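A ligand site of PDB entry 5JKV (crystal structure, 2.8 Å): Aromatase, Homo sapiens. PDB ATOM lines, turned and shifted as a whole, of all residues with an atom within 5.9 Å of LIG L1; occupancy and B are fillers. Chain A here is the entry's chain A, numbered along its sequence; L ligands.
An oxygen (O2) of LIG L1 is in hydrogen-bond range of the backbone NH of Met 374. NH1 of Arg 115 is in hydrogen-bond range of O2 of LIG L1. An oxygen (O1) of LG2 L2 lies within salt-bridge range of the guanidinium group of Arg 115 (2.7 Å). The guanidinium group (NH2) of Arg 375 lies within salt-bridge range of an oxygen (O2) of LG2 L2, at 2.8 Å.
NH1 of Arg 115 sits at hydrogen-bond distance from O of Met 374 (3.0 Å). The backbone carbonyl oxygen (O) of Ile 133 sits at hydrogen-bond distance from the guanidinium group (NE) of Arg 115, 2.8 Å away. The backbone carbonyl oxygen of Ala 306 is in hydrogen-bond range of the side-chain hydroxyl of Thr 310 (2.6 Å). The side-chain carboxylate of Glu 302 sits at hydrogen-bond distance from the backbone NH of Ile 133 (3.1 Å).
The side-chain carboxylate (OD2) of Asp 309 lies close to an oxygen (O1) of LIG L1, at 2.9 Å. Residues that only touch LIG L1: Ala 306 (3.4 Å), Leu 372 (3.4 Å), Trp 224 (3.6 Å), Val 370 (3.6 Å), Leu 477 (3.6 Å), Thr 310 (3.6 Å), Ile 133 (3.7 Å), Val 373 (3.7 Å), Ile 305 (3.8 Å) and Phe 134 (3.96 Å). Hydrophobic or aromatic side chains within 4 Å of LIG L1: Ile 133, Phe 134, Trp 224, Ile 305, Ala 306, Val 370, Leu 372, Met 374 and Leu 477. 13 residues have an atom within 4 Å of LIG L1: Arg 115, Ile 133, Phe 134, Trp 224, Ile 305, Ala 306, Asp 309, Thr 310, Val 370, Leu 372, Val 373, Met 374 and Leu 477.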
ATOM      1  N   ARG A 115      -3.577  22.283   8.430  1.00  0.00           N
ATOM      2  CA  ARG A 115      -4.958  21.775   8.463  1.00  0.00           C
ATOM      3  C   ARG A 115      -5.103  20.832   7.267  1.00  0.00           C
ATOM      4  O   ARG A 115      -4.095  20.380   6.698  1.00  0.00           O
ATOM      5  CB  ARG A 115      -5.979  22.923   8.398  1.00  0.00           C
ATOM      6  CG  ARG A 115      -5.685  24.080   9.331  1.00  0.00           C
ATOM      7  CD  ARG A 115      -6.936  24.820   9.755  1.00  0.00           C
ATOM      8  NE  ARG A 115      -6.591  25.923  10.639  1.00  0.00           N
ATOM      9  CZ  ARG A 115      -6.472  25.839  11.969  1.00  0.00           C
ATOM     10  NH1 ARG A 115      -6.691  24.686  12.600  1.00  0.00           N
ATOM     11  NH2 ARG A 115      -6.134  26.907  12.667  1.00  0.00           N
ATOM     12  N   ILE A 133      -5.941  30.783   7.286  1.00  0.00           N
ATOM     13  CA  ILE A 133      -6.908  29.890   7.958  1.00  0.00           C
ATOM     14  C   ILE A 133      -6.757  28.437   7.495  1.00  0.00           C
ATOM     15  O   ILE A 133      -6.483  27.560   8.309  1.00  0.00           O
ATOM     16  CB  ILE A 133      -8.381  30.375   7.859  1.00  0.00           C
ATOM     17  CG1 ILE A 133      -8.520  31.824   8.340  1.00  0.00           C
ATOM     18  CG2 ILE A 133      -9.290  29.488   8.689  1.00  0.00           C
ATOM     19  CD1 ILE A 133      -9.823  32.492   7.943  1.00  0.00           C
ATOM     20  N   PHE A 134      -6.913  28.207   6.194  1.00  0.00           N
ATOM     21  CA  PHE A 134      -6.737  26.871   5.616  1.00  0.00           C
ATOM     22  C   PHE A 134      -5.576  26.793   4.610  1.00  0.00           C
ATOM     23  O   PHE A 134      -5.591  25.986   3.671  1.00  0.00           O
ATOM     24  CB  PHE A 134      -8.066  26.345   5.029  1.00  0.00           C
ATOM     25  CG  PHE A 134      -8.949  25.665   6.042  1.00  0.00           C
ATOM     26  CD1 PHE A 134      -9.848  26.410   6.812  1.00  0.00           C
ATOM     27  CD2 PHE A 134      -8.873  24.289   6.240  1.00  0.00           C
ATOM     28  CE1 PHE A 134     -10.655  25.788   7.757  1.00  0.00           C
ATOM     29  CE2 PHE A 134      -9.670  23.657   7.187  1.00  0.00           C
ATOM     30  CZ  PHE A 134     -10.572  24.406   7.945  1.00  0.00           C
ATOM     31  N   PHE A 221     -19.150  31.929   3.666  1.00  0.00           N
ATOM     32  CA  PHE A 221     -19.067  30.893   4.676  1.00  0.00           C
ATOM     33  C   PHE A 221     -19.802  29.625   4.267  1.00  0.00           C
ATOM     34  O   PHE A 221     -19.296  28.524   4.500  1.00  0.00           O
ATOM     35  CB  PHE A 221     -19.533  31.355   6.059  1.00  0.00           C
ATOM     36  CG  PHE A 221     -19.310  30.321   7.129  1.00  0.00           C
ATOM     37  CD1 PHE A 221     -18.069  30.215   7.776  1.00  0.00           C
ATOM     38  CD2 PHE A 221     -20.330  29.423   7.476  1.00  0.00           C
ATOM     39  CE1 PHE A 221     -17.857  29.236   8.749  1.00  0.00           C
ATOM     40  CE2 PHE A 221     -20.118  28.444   8.449  1.00  0.00           C
ATOM     41  CZ  PHE A 221     -18.882  28.351   9.086  1.00  0.00           C
ATOM     42  N   TRP A 224     -17.588  27.880   1.712  1.00  0.00           N
ATOM     43  CA  TRP A 224     -16.496  27.324   2.494  1.00  0.00           C
ATOM     44  C   TRP A 224     -16.915  26.033   3.201  1.00  0.00           C
ATOM     45  O   TRP A 224     -16.292  24.987   3.001  1.00  0.00           O
ATOM     46  CB  TRP A 224     -15.994  28.404   3.464  1.00  0.00           C
ATOM     47  CG  TRP A 224     -14.886  28.048   4.445  1.00  0.00           C
ATOM     48  CD1 TRP A 224     -14.124  26.907   4.478  1.00  0.00           C
ATOM     49  CD2 TRP A 224     -14.396  28.873   5.504  1.00  0.00           C
ATOM     50  NE1 TRP A 224     -13.217  26.961   5.502  1.00  0.00           N
ATOM     51  CE2 TRP A 224     -13.358  28.158   6.151  1.00  0.00           C
ATOM     52  CE3 TRP A 224     -14.747  30.151   5.982  1.00  0.00           C
ATOM     53  CZ2 TRP A 224     -12.656  28.688   7.250  1.00  0.00           C
ATOM     54  CZ3 TRP A 224     -14.049  30.669   7.086  1.00  0.00           C
ATOM     55  CH2 TRP A 224     -13.014  29.931   7.699  1.00  0.00           C
ATOM     56  N   GLU A 302      -9.853  37.316   4.559  1.00  0.00           N
ATOM     57  CA  GLU A 302      -9.896  36.450   5.732  1.00  0.00           C
ATOM     58  C   GLU A 302      -9.979  37.228   7.052  1.00  0.00           C
ATOM     59  O   GLU A 302     -10.693  36.823   7.968  1.00  0.00           O
ATOM     60  CB  GLU A 302      -8.708  35.484   5.741  1.00  0.00           C
ATOM     61  CG  GLU A 302      -8.850  34.342   4.746  1.00  0.00           C
ATOM     62  CD  GLU A 302      -7.781  33.257   4.873  1.00  0.00           C
ATOM     63  OE1 GLU A 302      -6.947  33.306   5.803  1.00  0.00           O
ATOM     64  OE2 GLU A 302      -7.783  32.334   4.024  1.00  0.00           O
ATOM     65  N   ILE A 305     -13.663  38.611   7.377  1.00  0.00           N
ATOM     66  CA  ILE A 305     -14.733  37.643   7.609  1.00  0.00           C
ATOM     67  C   ILE A 305     -14.689  37.022   9.003  1.00  0.00           C
ATOM     68  O   ILE A 305     -15.721  36.606   9.530  1.00  0.00           O
ATOM     69  CB  ILE A 305     -14.797  36.524   6.523  1.00  0.00           C
ATOM     70  CG1 ILE A 305     -13.550  35.623   6.552  1.00  0.00           C
ATOM     71  CG2 ILE A 305     -15.047  37.126   5.145  1.00  0.00           C
ATOM     72  CD1 ILE A 305     -13.751  34.242   5.963  1.00  0.00           C
ATOM     73  N   ALA A 306     -13.496  36.986   9.597  1.00  0.00           N
ATOM     74  CA  ALA A 306     -13.238  36.219  10.815  1.00  0.00           C
ATOM     75  C   ALA A 306     -14.190  36.554  11.973  1.00  0.00           C
ATOM     76  O   ALA A 306     -14.859  35.655  12.493  1.00  0.00           O
ATOM     77  CB  ALA A 306     -11.781  36.344  11.245  1.00  0.00           C
ATOM     78  N   ALA A 307     -14.265  37.834  12.338  1.00  0.00           N
ATOM     79  CA  ALA A 307     -15.145  38.272  13.416  1.00  0.00           C
ATOM     80  C   ALA A 307     -16.656  38.143  13.097  1.00  0.00           C
ATOM     81  O   ALA A 307     -17.385  37.550  13.892  1.00  0.00           O
ATOM     82  CB  ALA A 307     -14.768  39.676  13.887  1.00  0.00           C
ATOM     83  N   ASP A 309     -17.932  35.943  11.259  1.00  0.00           N
ATOM     84  CA  ASP A 309     -18.202  34.503  11.215  1.00  0.00           C
ATOM     85  C   ASP A 309     -18.347  33.883  12.594  1.00  0.00           C
ATOM     86  O   ASP A 309     -19.241  33.056  12.810  1.00  0.00           O
ATOM     87  CB  ASP A 309     -17.116  33.756  10.423  1.00  0.00           C
ATOM     88  CG  ASP A 309     -17.288  33.892   8.909  1.00  0.00           C
ATOM     89  OD1 ASP A 309     -18.371  34.284   8.441  1.00  0.00           O
ATOM     90  OD2 ASP A 309     -16.323  33.591   8.184  1.00  0.00           O
ATOM     91  N   THR A 310     -17.481  34.279  13.526  1.00  0.00           N
ATOM     92  CA  THR A 310     -17.363  33.592  14.809  1.00  0.00           C
ATOM     93  C   THR A 310     -17.827  34.405  16.009  1.00  0.00           C
ATOM     94  O   THR A 310     -18.559  33.883  16.850  1.00  0.00           O
ATOM     95  CB  THR A 310     -15.931  33.074  15.055  1.00  0.00           C
ATOM     96  OG1 THR A 310     -14.967  34.039  14.588  1.00  0.00           O
ATOM     97  CG2 THR A 310     -15.719  31.784  14.319  1.00  0.00           C
ATOM     98  N   VAL A 370     -16.988  27.266  17.733  1.00  0.00           N
ATOM     99  CA  VAL A 370     -15.857  26.535  17.180  1.00  0.00           C
ATOM    100  C   VAL A 370     -15.549  25.358  18.119  1.00  0.00           C
ATOM    101  O   VAL A 370     -14.708  25.458  19.021  1.00  0.00           O
ATOM    102  CB  VAL A 370     -14.617  27.430  16.952  1.00  0.00           C
ATOM    103  CG1 VAL A 370     -13.584  26.709  16.112  1.00  0.00           C
ATOM    104  CG2 VAL A 370     -15.012  28.742  16.286  1.00  0.00           C
ATOM    105  N   LEU A 372     -14.661  22.276  16.999  1.00  0.00           N
ATOM    106  CA  LEU A 372     -13.691  21.375  16.376  1.00  0.00           C
ATOM    107  C   LEU A 372     -12.562  22.094  15.657  1.00  0.00           C
ATOM    108  O   LEU A 372     -12.768  23.143  15.052  1.00  0.00           O
ATOM    109  CB  LEU A 372     -14.381  20.349  15.469  1.00  0.00           C
ATOM    110  CG  LEU A 372     -15.143  20.778  14.222  1.00  0.00           C
ATOM    111  CD1 LEU A 372     -14.289  20.726  12.968  1.00  0.00           C
ATOM    112  CD2 LEU A 372     -16.337  19.857  14.056  1.00  0.00           C
ATOM    113  N   VAL A 373     -11.366  21.503  15.749  1.00  0.00           N
ATOM    114  CA  VAL A 373     -10.158  22.040  15.125  1.00  0.00           C
ATOM    115  C   VAL A 373      -9.578  20.989  14.169  1.00  0.00           C
ATOM    116  O   VAL A 373      -9.365  19.840  14.563  1.00  0.00           O
ATOM    117  CB  VAL A 373      -9.097  22.450  16.179  1.00  0.00           C
ATOM    118  CG1 VAL A 373      -7.825  22.961  15.524  1.00  0.00           C
ATOM    119  CG2 VAL A 373      -9.651  23.505  17.128  1.00  0.00           C
ATOM    120  N   MET A 374      -9.344  21.387  12.927  1.00  0.00           N
ATOM    121  CA  MET A 374      -8.788  20.498  11.902  1.00  0.00           C
ATOM    122  C   MET A 374      -7.280  20.697  11.757  1.00  0.00           C
ATOM    123  O   MET A 374      -6.808  21.814  11.580  1.00  0.00           O
ATOM    124  CB  MET A 374      -9.493  20.707  10.567  1.00  0.00           C
ATOM    125  CG  MET A 374     -10.948  20.250  10.572  1.00  0.00           C
ATOM    126  SD  MET A 374     -11.897  20.835   9.157  1.00  0.00           S
ATOM    127  CE  MET A 374     -11.204  19.832   7.836  1.00  0.00           C
ATOM    128  N   ARG A 375      -6.541  19.584  11.870  1.00  0.00           N
ATOM    129  CA  ARG A 375      -5.080  19.576  11.736  1.00  0.00           C
ATOM    130  C   ARG A 375      -4.566  18.432  10.830  1.00  0.00           C
ATOM    131  O   ARG A 375      -5.333  17.552  10.436  1.00  0.00           O
ATOM    132  CB  ARG A 375      -4.394  19.511  13.109  1.00  0.00           C
ATOM    133  CG  ARG A 375      -4.710  20.640  14.091  1.00  0.00           C
ATOM    134  CD  ARG A 375      -4.224  22.006  13.607  1.00  0.00           C
ATOM    135  NE  ARG A 375      -4.186  23.002  14.672  1.00  0.00           N
ATOM    136  CZ  ARG A 375      -3.105  23.294  15.394  1.00  0.00           C
ATOM    137  NH1 ARG A 375      -1.954  22.657  15.165  1.00  0.00           N
ATOM    138  NH2 ARG A 375      -3.162  24.215  16.341  1.00  0.00           N
ATOM    139  N   LEU A 477     -19.253  22.724   9.941  1.00  0.00           N
ATOM    140  CA  LEU A 477     -17.921  23.322  10.093  1.00  0.00           C
ATOM    141  C   LEU A 477     -17.807  24.058  11.431  1.00  0.00           C
ATOM    142  O   LEU A 477     -16.754  24.035  12.067  1.00  0.00           O
ATOM    143  CB  LEU A 477     -17.616  24.296   8.954  1.00  0.00           C
ATOM    144  CG  LEU A 477     -16.216  24.489   8.342  1.00  0.00           C
ATOM    145  CD1 LEU A 477     -15.920  25.974   8.185  1.00  0.00           C
ATOM    146  CD2 LEU A 477     -15.074  23.797   9.071  1.00  0.00           C
ATOM    147  N   SER A 478     -18.890  24.724  11.821  1.00  0.00           N
ATOM    148  CA  SER A 478     -19.026  25.318  13.143  1.00  0.00           C
ATOM    149  C   SER A 478     -20.402  24.973  13.707  1.00  0.00           C
ATOM    150  O   SER A 478     -21.252  24.416  12.996  1.00  0.00           O
ATOM    151  CB  SER A 478     -18.800  26.830  13.087  1.00  0.00           C
ATOM    152  OG  SER A 478     -19.849  27.497  12.417  1.00  0.00           O
HETATM  153  C1  LIG L   1     -11.598  31.077  11.317  1.00  0.00           C
HETATM  154  C2  LIG L   1     -12.498  30.036  12.027  1.00  0.00           C
HETATM  155  C3  LIG L   1     -10.538  28.300  11.969  1.00  0.00           C
HETATM  156  C4  LIG L   1     -10.080  26.858  11.694  1.00  0.00           C
HETATM  157  C5  LIG L   1     -11.040  25.850  12.331  1.00  0.00           C
HETATM  158  C6  LIG L   1     -12.428  26.099  11.741  1.00  0.00           C
HETATM  159  C7  LIG L   1     -13.242  24.823  11.998  1.00  0.00           C
HETATM  160  C8  LIG L   1     -12.222  23.716  11.712  1.00  0.00           C
HETATM  161  C9  LIG L   1     -10.887  24.414  11.923  1.00  0.00           C
HETATM  162  C10 LIG L   1     -10.922  25.858  13.862  1.00  0.00           C
HETATM  163  C11 LIG L   1     -12.387  30.257  13.540  1.00  0.00           C
HETATM  164  C12 LIG L   1     -12.192  32.478  11.169  1.00  0.00           C
HETATM  165  C13 LIG L   1     -13.546  32.344  10.506  1.00  0.00           C
HETATM  166  C14 LIG L   1     -14.445  31.237  10.915  1.00  0.00           C
HETATM  167  C15 LIG L   1     -13.967  30.162  11.589  1.00  0.00           C
HETATM  168  C16 LIG L   1     -14.966  29.059  11.892  1.00  0.00           C
HETATM  169  C17 LIG L   1     -14.395  27.717  11.451  1.00  0.00           C
HETATM  170  C18 LIG L   1     -13.011  27.481  12.067  1.00  0.00           C
HETATM  171  C19 LIG L   1     -12.020  28.600  11.620  1.00  0.00           C
HETATM  172  O1  LIG L   1     -13.874  33.134   9.642  1.00  0.00           O
HETATM  173  O2  LIG L   1      -9.802  23.857  11.790  1.00  0.00           O
HETATM  174  C1  LG2 L   2      -8.163  30.000  14.224  1.00  0.00           C
HETATM  175  C2  LG2 L   2     -11.435  30.121  17.768  1.00  0.00           C
HETATM  176  C3  LG2 L   2     -12.041  34.832  16.951  1.00  0.00           C
HETATM  177  C4  LG2 L   2      -8.691  34.792  13.494  1.00  0.00           C
HETATM  178  C5  LG2 L   2      -8.956  29.633  15.276  1.00  0.00           C
HETATM  179  C6  LG2 L   2      -8.993  28.311  15.886  1.00  0.00           C
HETATM  180  C7  LG2 L   2      -9.892  28.353  16.879  1.00  0.00           C
HETATM  181  C8  LG2 L   2     -10.445  29.689  16.916  1.00  0.00           C
HETATM  182  C9  LG2 L   2     -10.271  27.182  17.821  1.00  0.00           C
HETATM  183  C10 LG2 L   2      -8.119  27.100  15.489  1.00  0.00           C
HETATM  184  C11 LG2 L   2      -6.769  27.241  16.200  1.00  0.00           C
HETATM  185  C12 LG2 L   2      -5.961  25.967  16.168  1.00  0.00           C
HETATM  186  O1  LG2 L   2      -5.857  25.319  15.075  1.00  0.00           O
HETATM  187  O2  LG2 L   2      -5.405  25.590  17.235  1.00  0.00           O
HETATM  188  C13 LG2 L   2     -11.961  31.386  17.773  1.00  0.00           C
HETATM  189  C14 LG2 L   2     -13.136  31.835  18.508  1.00  0.00           C
HETATM  190  C15 LG2 L   2     -13.288  33.137  18.275  1.00  0.00           C
HETATM  191  C16 LG2 L   2     -12.221  33.547  17.391  1.00  0.00           C
HETATM  192  C17 LG2 L   2     -14.031  30.937  19.391  1.00  0.00           C
HETATM  193  C18 LG2 L   2     -14.387  34.113  18.786  1.00  0.00           C
HETATM  194  C19 LG2 L   2     -15.048  33.888  19.916  1.00  0.00           C
HETATM  195  C20 LG2 L   2     -11.165  35.241  15.976  1.00  0.00           C
HETATM  196  C21 LG2 L   2     -10.996  36.602  15.518  1.00  0.00           C
HETATM  197  C22 LG2 L   2     -10.053  36.591  14.550  1.00  0.00           C
HETATM  198  C23 LG2 L   2      -9.625  35.219  14.389  1.00  0.00           C
HETATM  199  C24 LG2 L   2     -11.762  37.819  16.067  1.00  0.00           C
HETATM  200  C25 LG2 L   2      -9.500  37.789  13.746  1.00  0.00           C
HETATM  201  C26 LG2 L   2     -10.283  38.820  13.371  1.00  0.00           C
HETATM  202  C27 LG2 L   2      -8.278  33.493  13.324  1.00  0.00           C
HETATM  203  C28 LG2 L   2      -7.367  33.058  12.290  1.00  0.00           C
HETATM  204  C29 LG2 L   2      -7.197  31.555  12.502  1.00  0.00           C
HETATM  205  C30 LG2 L   2      -8.028  31.249  13.660  1.00  0.00           C
HETATM  206  C31 LG2 L   2      -6.708  33.929  11.196  1.00  0.00           C
HETATM  207  C32 LG2 L   2      -6.303  30.605  11.671  1.00  0.00           C
HETATM  208  C33 LG2 L   2      -4.951  30.547  12.389  1.00  0.00           C
HETATM  209  C34 LG2 L   2      -3.934  29.715  11.648  1.00  0.00           C
HETATM  210  O3  LG2 L   2      -2.722  30.075  11.659  1.00  0.00           O
HETATM  211  O4  LG2 L   2      -4.317  28.673  11.029  1.00  0.00           O
HETATM  212  N1  LG2 L   2      -9.839  30.439  15.943  1.00  0.00           N
HETATM  213  N2  LG2 L   2     -11.429  32.459  17.120  1.00  0.00           N
HETATM  214  N3  LG2 L   2     -10.306  34.417  15.288  1.00  0.00           N
HETATM  215  N4  LG2 L   2      -8.644  32.407  14.109  1.00  0.00           N
HETATM  216 FE1  LG2 L   2     -10.045  32.436  15.659  1.00  0.00          FE
